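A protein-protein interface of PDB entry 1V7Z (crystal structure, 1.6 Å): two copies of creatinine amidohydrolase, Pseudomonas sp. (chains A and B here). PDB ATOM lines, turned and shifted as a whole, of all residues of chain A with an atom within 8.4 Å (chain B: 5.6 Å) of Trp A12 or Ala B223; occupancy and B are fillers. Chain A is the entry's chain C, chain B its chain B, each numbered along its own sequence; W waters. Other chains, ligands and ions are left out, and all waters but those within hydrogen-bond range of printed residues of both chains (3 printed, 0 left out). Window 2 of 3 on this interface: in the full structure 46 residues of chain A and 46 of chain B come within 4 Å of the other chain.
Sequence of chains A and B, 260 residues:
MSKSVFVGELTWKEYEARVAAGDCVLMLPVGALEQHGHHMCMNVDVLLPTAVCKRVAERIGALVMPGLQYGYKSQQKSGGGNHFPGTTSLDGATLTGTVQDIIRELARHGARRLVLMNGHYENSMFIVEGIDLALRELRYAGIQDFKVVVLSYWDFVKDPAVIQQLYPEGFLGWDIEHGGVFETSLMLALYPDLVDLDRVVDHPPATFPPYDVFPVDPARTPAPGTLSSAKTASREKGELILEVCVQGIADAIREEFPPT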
ATOM      1  N   VAL A   7      -7.029  -7.423 -12.616  1.00  0.00           N
ATOM      2  CA  VAL A   7      -7.236  -8.387 -11.536  1.00  0.00           C
ATOM      3  C   VAL A   7      -6.453  -9.679 -11.777  1.00  0.00           C
ATOM      4  O   VAL A   7      -5.894 -10.247 -10.848  1.00  0.00           O
ATOM      5  CB  VAL A   7      -8.757  -8.708 -11.355  1.00  0.00           C
ATOM      6  CG1 VAL A   7      -8.980  -9.845 -10.351  1.00  0.00           C
ATOM      7  CG2 VAL A   7      -9.517  -7.460 -10.928  1.00  0.00           C
ATOM      8  N   GLY A   8      -6.392 -10.133 -13.024  1.00  0.00           N
ATOM      9  CA  GLY A   8      -5.666 -11.344 -13.350  1.00  0.00           C
ATOM     10  C   GLY A   8      -4.179 -11.265 -13.047  1.00  0.00           C
ATOM     11  O   GLY A   8      -3.546 -12.285 -12.818  1.00  0.00           O
ATOM     12  N   GLU A   9      -3.630 -10.056 -13.065  1.00  0.00           N
ATOM     13  CA  GLU A   9      -2.204  -9.830 -12.823  1.00  0.00           C
ATOM     14  C   GLU A   9      -1.877  -9.504 -11.356  1.00  0.00           C
ATOM     15  O   GLU A   9      -0.716  -9.255 -11.019  1.00  0.00           O
ATOM     16  CB  GLU A   9      -1.692  -8.728 -13.757  1.00  0.00           C
ATOM     17  CG  GLU A   9      -1.739  -9.135 -15.219  1.00  0.00           C
ATOM     18  CD  GLU A   9      -1.196  -8.100 -16.191  1.00  0.00           C
ATOM     19  OE1 GLU A   9      -1.096  -6.903 -15.842  1.00  0.00           O
ATOM     20  OE2 GLU A   9      -0.883  -8.495 -17.331  1.00  0.00           O
ATOM     21  N   LEU A  10      -2.887  -9.522 -10.491  1.00  0.00           N
ATOM     22  CA  LEU A  10      -2.700  -9.332  -9.053  1.00  0.00           C
ATOM     23  C   LEU A  10      -2.682 -10.666  -8.325  1.00  0.00           C
ATOM     24  O   LEU A  10      -3.201 -11.658  -8.831  1.00  0.00           O
ATOM     25  CB  LEU A  10      -3.827  -8.483  -8.472  1.00  0.00           C
ATOM     26  CG  LEU A  10      -4.061  -7.086  -9.047  1.00  0.00           C
ATOM     27  CD1 LEU A  10      -5.101  -6.372  -8.208  1.00  0.00           C
ATOM     28  CD2 LEU A  10      -2.769  -6.288  -9.124  1.00  0.00           C
ATOM     29  N   THR A  11      -2.078 -10.694  -7.135  1.00  0.00           N
ATOM     30  CA  THR A  11      -2.222 -11.838  -6.241  1.00  0.00           C
ATOM     31  C   THR A  11      -3.554 -11.693  -5.539  1.00  0.00           C
ATOM     32  O   THR A  11      -4.137 -10.608  -5.510  1.00  0.00           O
ATOM     33  CB  THR A  11      -1.108 -11.896  -5.173  1.00  0.00           C
ATOM     34  OG1 THR A  11      -1.263 -10.805  -4.255  1.00  0.00           O
ATOM     35  CG2 THR A  11       0.262 -11.716  -5.787  1.00  0.00           C
ATOM     36  N   TRP A  12      -4.036 -12.772  -4.941  1.00  0.00           N
ATOM     37  CA  TRP A  12      -5.290 -12.700  -4.214  1.00  0.00           C
ATOM     38  C   TRP A  12      -5.216 -11.773  -3.002  1.00  0.00           C
ATOM     39  O   TRP A  12      -6.207 -11.158  -2.641  1.00  0.00           O
ATOM     40  CB  TRP A  12      -5.791 -14.089  -3.833  1.00  0.00           C
ATOM     41  CG  TRP A  12      -5.085 -14.791  -2.707  1.00  0.00           C
ATOM     42  CD1 TRP A  12      -4.055 -15.681  -2.813  1.00  0.00           C
ATOM     43  CD2 TRP A  12      -5.409 -14.715  -1.319  1.00  0.00           C
ATOM     44  NE1 TRP A  12      -3.707 -16.152  -1.569  1.00  0.00           N
ATOM     45  CE2 TRP A  12      -4.525 -15.577  -0.633  1.00  0.00           C
ATOM     46  CE3 TRP A  12      -6.357 -13.999  -0.578  1.00  0.00           C
ATOM     47  CZ2 TRP A  12      -4.560 -15.739   0.756  1.00  0.00           C
ATOM     48  CZ3 TRP A  12      -6.391 -14.163   0.808  1.00  0.00           C
ATOM     49  CH2 TRP A  12      -5.495 -15.028   1.454  1.00  0.00           C
ATOM     50  N   LYS A  13      -4.035 -11.655  -2.401  1.00  0.00           N
ATOM     51  CA  LYS A  13      -3.855 -10.748  -1.270  1.00  0.00           C
ATOM     52  C   LYS A  13      -3.935  -9.282  -1.694  1.00  0.00           C
ATOM     53  O   LYS A  13      -4.508  -8.464  -0.981  1.00  0.00           O
ATOM     54  CB  LYS A  13      -2.520 -11.022  -0.573  1.00  0.00           C
ATOM     55  CG  LYS A  13      -2.421 -12.404   0.070  1.00  0.00           C
ATOM     56  CD  LYS A  13      -3.183 -12.481   1.382  1.00  0.00           C
ATOM     57  CE  LYS A  13      -2.506 -11.679   2.480  1.00  0.00           C
ATOM     58  NZ  LYS A  13      -2.690 -12.308   3.825  1.00  0.00           N
ATOM     59  N   GLU A  14      -3.359  -8.962  -2.848  1.00  0.00           N
ATOM     60  CA  GLU A  14      -3.405  -7.608  -3.403  1.00  0.00           C
ATOM     61  C   GLU A  14      -4.847  -7.245  -3.753  1.00  0.00           C
ATOM     62  O   GLU A  14      -5.326  -6.161  -3.428  1.00  0.00           O
ATOM     63  CB  GLU A  14      -2.502  -7.492  -4.636  1.00  0.00           C
ATOM     64  CG  GLU A  14      -1.013  -7.571  -4.295  1.00  0.00           C
ATOM     65  CD  GLU A  14      -0.087  -7.765  -5.490  1.00  0.00           C
ATOM     66  OE1 GLU A  14       1.134  -7.531  -5.316  1.00  0.00           O
ATOM     67  OE2 GLU A  14      -0.527  -8.158  -6.592  1.00  0.00           O
ATOM     68  N   TYR A  15      -5.546  -8.178  -4.394  1.00  0.00           N
ATOM     69  CA  TYR A  15      -6.953  -7.989  -4.723  1.00  0.00           C
ATOM     70  C   TYR A  15      -7.797  -7.807  -3.462  1.00  0.00           C
ATOM     71  O   TYR A  15      -8.609  -6.901  -3.383  1.00  0.00           O
ATOM     72  CB  TYR A  15      -7.471  -9.186  -5.533  1.00  0.00           C
ATOM     73  CG  TYR A  15      -8.955  -9.124  -5.837  1.00  0.00           C
ATOM     74  CD1 TYR A  15      -9.431  -8.374  -6.903  1.00  0.00           C
ATOM     75  CD2 TYR A  15      -9.876  -9.814  -5.053  1.00  0.00           C
ATOM     76  CE1 TYR A  15     -10.782  -8.313  -7.180  1.00  0.00           C
ATOM     77  CE2 TYR A  15     -11.234  -9.757  -5.319  1.00  0.00           C
ATOM     78  CZ  TYR A  15     -11.681  -9.005  -6.383  1.00  0.00           C
ATOM     79  OH  TYR A  15     -13.028  -8.965  -6.645  1.00  0.00           O
ATOM     80  N   GLU A  16      -7.597  -8.675  -2.479  1.00  0.00           N
ATOM     81  CA  GLU A  16      -8.324  -8.609  -1.215  1.00  0.00           C
ATOM     82  C   GLU A  16      -8.138  -7.253  -0.533  1.00  0.00           C
ATOM     83  O   GLU A  16      -9.087  -6.695   0.010  1.00  0.00           O
ATOM     84  CB  GLU A  16      -7.850  -9.723  -0.278  1.00  0.00           C
ATOM     85  CG  GLU A  16      -8.554  -9.762   1.069  1.00  0.00           C
ATOM     86  CD  GLU A  16      -7.959 -10.792   2.009  1.00  0.00           C
ATOM     87  OE1 GLU A  16      -8.735 -11.546   2.633  1.00  0.00           O
ATOM     88  OE2 GLU A  16      -6.715 -10.854   2.121  1.00  0.00           O
ATOM     89  N   ALA A  17      -6.913  -6.741  -0.566  1.00  0.00           N
ATOM     90  CA  ALA A  17      -6.596  -5.450   0.048  1.00  0.00           C
ATOM     91  C   ALA A  17      -7.334  -4.304  -0.648  1.00  0.00           C
ATOM     92  O   ALA A  17      -7.837  -3.393   0.018  1.00  0.00           O
ATOM     93  CB  ALA A  17      -5.083  -5.207   0.033  1.00  0.00           C
ATOM     94  N   ARG A  18      -7.415  -4.356  -1.978  1.00  0.00           N
ATOM     95  CA  ARG A  18      -8.102  -3.316  -2.743  1.00  0.00           C
ATOM     96  C   ARG A  18      -9.600  -3.309  -2.474  1.00  0.00           C
ATOM     97  O   ARG A  18     -10.209  -2.247  -2.372  1.00  0.00           O
ATOM     98  CB  ARG A  18      -7.831  -3.464  -4.243  1.00  0.00           C
ATOM     99  CG  ARG A  18      -6.395  -3.143  -4.633  1.00  0.00           C
ATOM    100  CD  ARG A  18      -6.010  -1.678  -4.448  1.00  0.00           C
ATOM    101  NE  ARG A  18      -6.810  -0.810  -5.308  1.00  0.00           N
ATOM    102  CZ  ARG A  18      -6.548  -0.565  -6.588  1.00  0.00           C
ATOM    103  NH1 ARG A  18      -5.489  -1.091  -7.186  1.00  0.00           N
ATOM    104  NH2 ARG A  18      -7.352   0.229  -7.275  1.00  0.00           N
ATOM    105  N   VAL A  19     -10.194  -4.489  -2.341  1.00  0.00           N
ATOM    106  CA  VAL A  19     -11.610  -4.584  -2.017  1.00  0.00           C
ATOM    107  C   VAL A  19     -11.860  -4.120  -0.577  1.00  0.00           C
ATOM    108  O   VAL A  19     -12.886  -3.505  -0.289  1.00  0.00           O
ATOM    109  CB  VAL A  19     -12.136  -6.009  -2.228  1.00  0.00           C
ATOM    110  CG1 VAL A  19     -13.579  -6.137  -1.746  1.00  0.00           C
ATOM    111  CG2 VAL A  19     -12.021  -6.389  -3.708  1.00  0.00           C
ATOM    112  N   GLN B  35      -7.043 -17.669  -7.126  1.00  0.00           N
ATOM    113  CA  GLN B  35      -5.919 -17.408  -6.232  1.00  0.00           C
ATOM    114  C   GLN B  35      -4.801 -18.427  -6.479  1.00  0.00           C
ATOM    115  O   GLN B  35      -5.054 -19.617  -6.683  1.00  0.00           O
ATOM    116  CB  GLN B  35      -6.371 -17.449  -4.768  1.00  0.00           C
ATOM    117  CG  GLN B  35      -6.768 -18.832  -4.242  1.00  0.00           C
ATOM    118  CD  GLN B  35      -5.590 -19.669  -3.774  1.00  0.00           C
ATOM    119  OE1 GLN B  35      -4.495 -19.150  -3.565  1.00  0.00           O
ATOM    120  NE2 GLN B  35      -5.807 -20.973  -3.644  1.00  0.00           N
ATOM    121  N   HIS B  36      -3.566 -17.943  -6.464  1.00  0.00           N
ATOM    122  CA  HIS B  36      -2.392 -18.792  -6.593  1.00  0.00           C
ATOM    123  C   HIS B  36      -1.319 -18.351  -5.601  1.00  0.00           C
ATOM    124  O   HIS B  36      -0.167 -18.137  -5.975  1.00  0.00           O
ATOM    125  CB  HIS B  36      -1.853 -18.736  -8.011  1.00  0.00           C
ATOM    126  CG  HIS B  36      -2.533 -19.674  -8.957  1.00  0.00           C
ATOM    127  ND1 HIS B  36      -3.660 -19.320  -9.670  1.00  0.00           N
ATOM    128  CD2 HIS B  36      -2.238 -20.945  -9.321  1.00  0.00           C
ATOM    129  CE1 HIS B  36      -4.029 -20.335 -10.431  1.00  0.00           C
ATOM    130  NE2 HIS B  36      -3.185 -21.334 -10.240  1.00  0.00           N
ATOM    131  N   GLY B  37      -1.720 -18.202  -4.346  1.00  0.00           N
ATOM    132  CA  GLY B  37      -0.778 -17.916  -3.277  1.00  0.00           C
ATOM    133  C   GLY B  37      -0.398 -16.455  -3.159  1.00  0.00           C
ATOM    134  O   GLY B  37      -0.979 -15.580  -3.799  1.00  0.00           O
ATOM    135  N   HIS B  38       0.596 -16.198  -2.312  1.00  0.00           N
ATOM    136  CA  HIS B  38       1.096 -14.849  -2.067  1.00  0.00           C
ATOM    137  C   HIS B  38       2.061 -14.339  -3.133  1.00  0.00           C
ATOM    138  O   HIS B  38       2.291 -13.134  -3.226  1.00  0.00           O
ATOM    139  CB  HIS B  38       1.812 -14.804  -0.710  1.00  0.00           C
ATOM    140  CG  HIS B  38       0.903 -14.959   0.465  1.00  0.00           C
ATOM    141  ND1 HIS B  38       1.234 -14.496   1.720  1.00  0.00           N
ATOM    142  CD2 HIS B  38      -0.318 -15.530   0.586  1.00  0.00           C
ATOM    143  CE1 HIS B  38       0.252 -14.766   2.562  1.00  0.00           C
ATOM    144  NE2 HIS B  38      -0.701 -15.395   1.899  1.00  0.00           N
ATOM    145  N   MET B  40       2.181 -15.112  -6.651  1.00  0.00           N
ATOM    146  CA  MET B  40       1.829 -15.303  -8.049  1.00  0.00           C
ATOM    147  C   MET B  40       0.447 -14.737  -8.332  1.00  0.00           C
ATOM    148  O   MET B  40      -0.393 -14.667  -7.444  1.00  0.00           O
ATOM    149  CB  MET B  40       1.857 -16.796  -8.378  1.00  0.00           C
ATOM    150  CG  MET B  40       2.003 -17.114  -9.839  1.00  0.00           C
ATOM    151  SD  MET B  40       2.825 -18.692 -10.128  1.00  0.00           S
ATOM    152  CE  MET B  40       1.751 -19.854  -9.321  1.00  0.00           C
ATOM    153  N   MET B  42      -3.343 -14.231 -10.474  1.00  0.00           N
ATOM    154  CA  MET B  42      -4.539 -15.086 -10.491  1.00  0.00           C
ATOM    155  C   MET B  42      -4.968 -15.619 -11.865  1.00  0.00           C
ATOM    156  O   MET B  42      -5.849 -16.476 -11.931  1.00  0.00           O
ATOM    157  CB  MET B  42      -5.698 -14.355  -9.821  1.00  0.00           C
ATOM    158  CG  MET B  42      -5.484 -14.154  -8.328  1.00  0.00           C
ATOM    159  SD  MET B  42      -6.880 -13.543  -7.452  1.00  0.00           S
ATOM    160  CE  MET B  42      -6.842 -11.823  -7.927  1.00  0.00           C
ATOM    161  N   PHE B  84     -11.837 -18.371  -1.174  1.00  0.00           N
ATOM    162  CA  PHE B  84     -10.812 -17.332  -1.303  1.00  0.00           C
ATOM    163  C   PHE B  84     -11.305 -16.115  -2.094  1.00  0.00           C
ATOM    164  O   PHE B  84     -12.088 -16.257  -3.038  1.00  0.00           O
ATOM    165  CB  PHE B  84      -9.558 -17.874  -1.989  1.00  0.00           C
ATOM    166  CG  PHE B  84      -8.642 -18.626  -1.075  1.00  0.00           C
ATOM    167  CD1 PHE B  84      -8.831 -19.980  -0.841  1.00  0.00           C
ATOM    168  CD2 PHE B  84      -7.577 -17.984  -0.460  1.00  0.00           C
ATOM    169  CE1 PHE B  84      -7.986 -20.682   0.004  1.00  0.00           C
ATOM    170  CE2 PHE B  84      -6.721 -18.685   0.376  1.00  0.00           C
ATOM    171  CZ  PHE B  84      -6.932 -20.034   0.613  1.00  0.00           C
ATOM    172  N   PRO B  85     -10.820 -14.926  -1.737  1.00  0.00           N
ATOM    173  CA  PRO B  85     -11.018 -13.728  -2.561  1.00  0.00           C
ATOM    174  C   PRO B  85     -10.341 -13.881  -3.921  1.00  0.00           C
ATOM    175  O   PRO B  85      -9.373 -14.630  -4.029  1.00  0.00           O
ATOM    176  CB  PRO B  85     -10.308 -12.616  -1.769  1.00  0.00           C
ATOM    177  CG  PRO B  85      -9.956 -13.181  -0.456  1.00  0.00           C
ATOM    178  CD  PRO B  85     -10.028 -14.649  -0.525  1.00  0.00           C
ATOM    179  N   GLY B  86     -10.837 -13.178  -4.939  1.00  0.00           N
ATOM    180  CA  GLY B  86     -10.191 -13.137  -6.234  1.00  0.00           C
ATOM    181  C   GLY B  86     -10.659 -14.243  -7.160  1.00  0.00           C
ATOM    182  O   GLY B  86     -11.016 -13.988  -8.306  1.00  0.00           O
ATOM    183  N   THR B 221      -7.123 -25.746   4.418  1.00  0.00           N
ATOM    184  CA  THR B 221      -6.231 -25.307   3.345  1.00  0.00           C
ATOM    185  C   THR B 221      -5.095 -24.515   3.976  1.00  0.00           C
ATOM    186  O   THR B 221      -5.357 -23.703   4.862  1.00  0.00           O
ATOM    187  CB  THR B 221      -6.984 -24.367   2.374  1.00  0.00           C
ATOM    188  OG1 THR B 221      -8.089 -25.055   1.778  1.00  0.00           O
ATOM    189  CG2 THR B 221      -6.110 -23.963   1.190  1.00  0.00           C
ATOM    190  N   PRO B 222      -3.851 -24.711   3.532  1.00  0.00           N
ATOM    191  CA  PRO B 222      -2.756 -23.836   3.971  1.00  0.00           C
ATOM    192  C   PRO B 222      -3.122 -22.367   3.777  1.00  0.00           C
ATOM    193  O   PRO B 222      -3.677 -22.010   2.737  1.00  0.00           O
ATOM    194  CB  PRO B 222      -1.596 -24.246   3.063  1.00  0.00           C
ATOM    195  CG  PRO B 222      -1.869 -25.657   2.739  1.00  0.00           C
ATOM    196  CD  PRO B 222      -3.366 -25.759   2.618  1.00  0.00           C
ATOM    197  N   ALA B 223      -2.821 -21.532   4.768  1.00  0.00           N
ATOM    198  CA  ALA B 223      -3.267 -20.139   4.777  1.00  0.00           C
ATOM    199  C   ALA B 223      -2.984 -19.348   3.486  1.00  0.00           C
ATOM    200  O   ALA B 223      -3.839 -18.570   3.067  1.00  0.00           O
ATOM    201  CB  ALA B 223      -2.692 -19.397   5.992  1.00  0.00           C
ATOM    202  N   PRO B 224      -1.811 -19.515   2.871  1.00  0.00           N
ATOM    203  CA  PRO B 224      -1.489 -18.792   1.629  1.00  0.00           C
ATOM    204  C   PRO B 224      -2.312 -19.209   0.402  1.00  0.00           C
ATOM    205  O   PRO B 224      -2.330 -18.468  -0.566  1.00  0.00           O
ATOM    206  CB  PRO B 224      -0.008 -19.115   1.392  1.00  0.00           C
ATOM    207  CG  PRO B 224       0.478 -19.726   2.651  1.00  0.00           C
ATOM    208  CD  PRO B 224      -0.684 -20.358   3.309  1.00  0.00           C
ATOM    209  N   GLY B 225      -2.940 -20.378   0.439  1.00  0.00           N
ATOM    210  CA  GLY B 225      -3.792 -20.844  -0.649  1.00  0.00           C
ATOM    211  C   GLY B 225      -3.105 -21.842  -1.564  1.00  0.00           C
ATOM    212  O   GLY B 225      -3.760 -22.497  -2.370  1.00  0.00           O
HETATM  213  O   HOH W   1      -2.747 -15.779   3.680  1.00  0.00           O
HETATM  214  O   HOH W   2       0.660 -11.250  -2.229  1.00  0.00           O
HETATM  215  O   HOH W   3      -2.568 -15.232  -5.943  1.00  0.00           O
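No position is printed for both chains.
Printed residues of chain B within 4 Å of Gly A8: Met B42. Val A19 touches none of the printed residues of chain B. His B36 touches none of the printed residues of chain A. Printed residues of chain A within 4 Å of Gly B37: Thr A11 (3.9 Å) and Trp A12 (3.2 Å). Of the printed residues of chain A, Met B42 touches Val A7, Gly A8, Leu A10, Thr A11, Trp A12 and Tyr A15. Pro B224 touches just one residue of chain A: Trp A12. The nearest residue of chain B that does not touch Trp A12 is His B38 (4.04 Å).
Among the printed residues, pairs that only touch across the chains: Trp A12 with Gly B37 (3.2 Å), Thr A11 with Met B40 (3.4 Å), Val A7 with Met B42 (3.5 Å), Tyr A15 with Gly B86 (3.5 Å), Trp A12 with Gln B35 (3.5 Å), Thr A11 with His B38 (3.6 Å), Tyr A15 with Met B42 (3.6 Å), Trp A12 with Pro B85 (3.6 Å), Trp A12 with Phe B84 (3.7 Å), Glu A16 with Pro B85 (3.7 Å), Trp A12 with Met B42 (3.7 Å), Trp A12 with Ala B223 (3.7 Å), Lys A13 with His B38 (3.8 Å), Thr A11 with Met B42 (3.8 Å) and Thr A11 with Gly B37 (3.9 Å).
The indole nitrogen (NE1) of Trp A12 is in hydrogen-bond range of the backbone carbonyl oxygen (O) of Pro B224 (2.9 Å). The backbone NH (N) of Met B42 sits at hydrogen-bond distance from the backbone carbonyl oxygen (O) of Leu A10 (3.1 Å). O of Gly A8 sits at hydrogen-bond distance from N of Met B42, at 3.1 Å.
Printed residues of chain B that touch a printed residue of chain A: Gln B35, Gly B37, His B38, Met B40, Met B42, Phe B84, Pro B85, Gly B86, Ala B223 and Pro B224. Hydrophobic or aromatic side chains of chain B that line the printed part of chain A: His B38, Met B42, Phe B84 and Pro B85. Along chain B the printed residues that touch a printed residue of chain A span positions 35 to 224. Of the 13 printed residues of chain A, 8 touch a printed residue of chain B. Along chain A the printed residues that touch a printed residue of chain B span positions 7 to 16. Among the printed residues, no Asp or Glu carboxylate lies within 4 Å of a Lys or Arg side-chain nitrogen of the other chain.
OE2 of Glu A14 lies within hydrogen-bond range of N of Thr A11 (3.0 Å). NE2 of Gln B35 lies within hydrogen-bond range of O of Gly B225 (2.9 Å). The backbone NH of Gly B37 lies within hydrogen-bond range of the side-chain amide oxygen of Gln B35. The side-chain hydroxyl (OG1) of Thr A11 sits close to the backbone NH (N) of Lys A13, at 3.4 Å.
Water W2 lies within hydrogen-bond range of the backbone carbonyl oxygen of His B38 and the side-chain hydroxyl of Thr A11. Water W3 lies within hydrogen-bond range of O of Gly B37 (2.7 Å), O of Met B40 (2.7 Å), N of His B36 (2.9 Å) and N of Trp A12 (3.0 Å). Water W1 lies within hydrogen-bond range of NE2 of His B38, O of Ala B223 and NZ of Lys A13.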
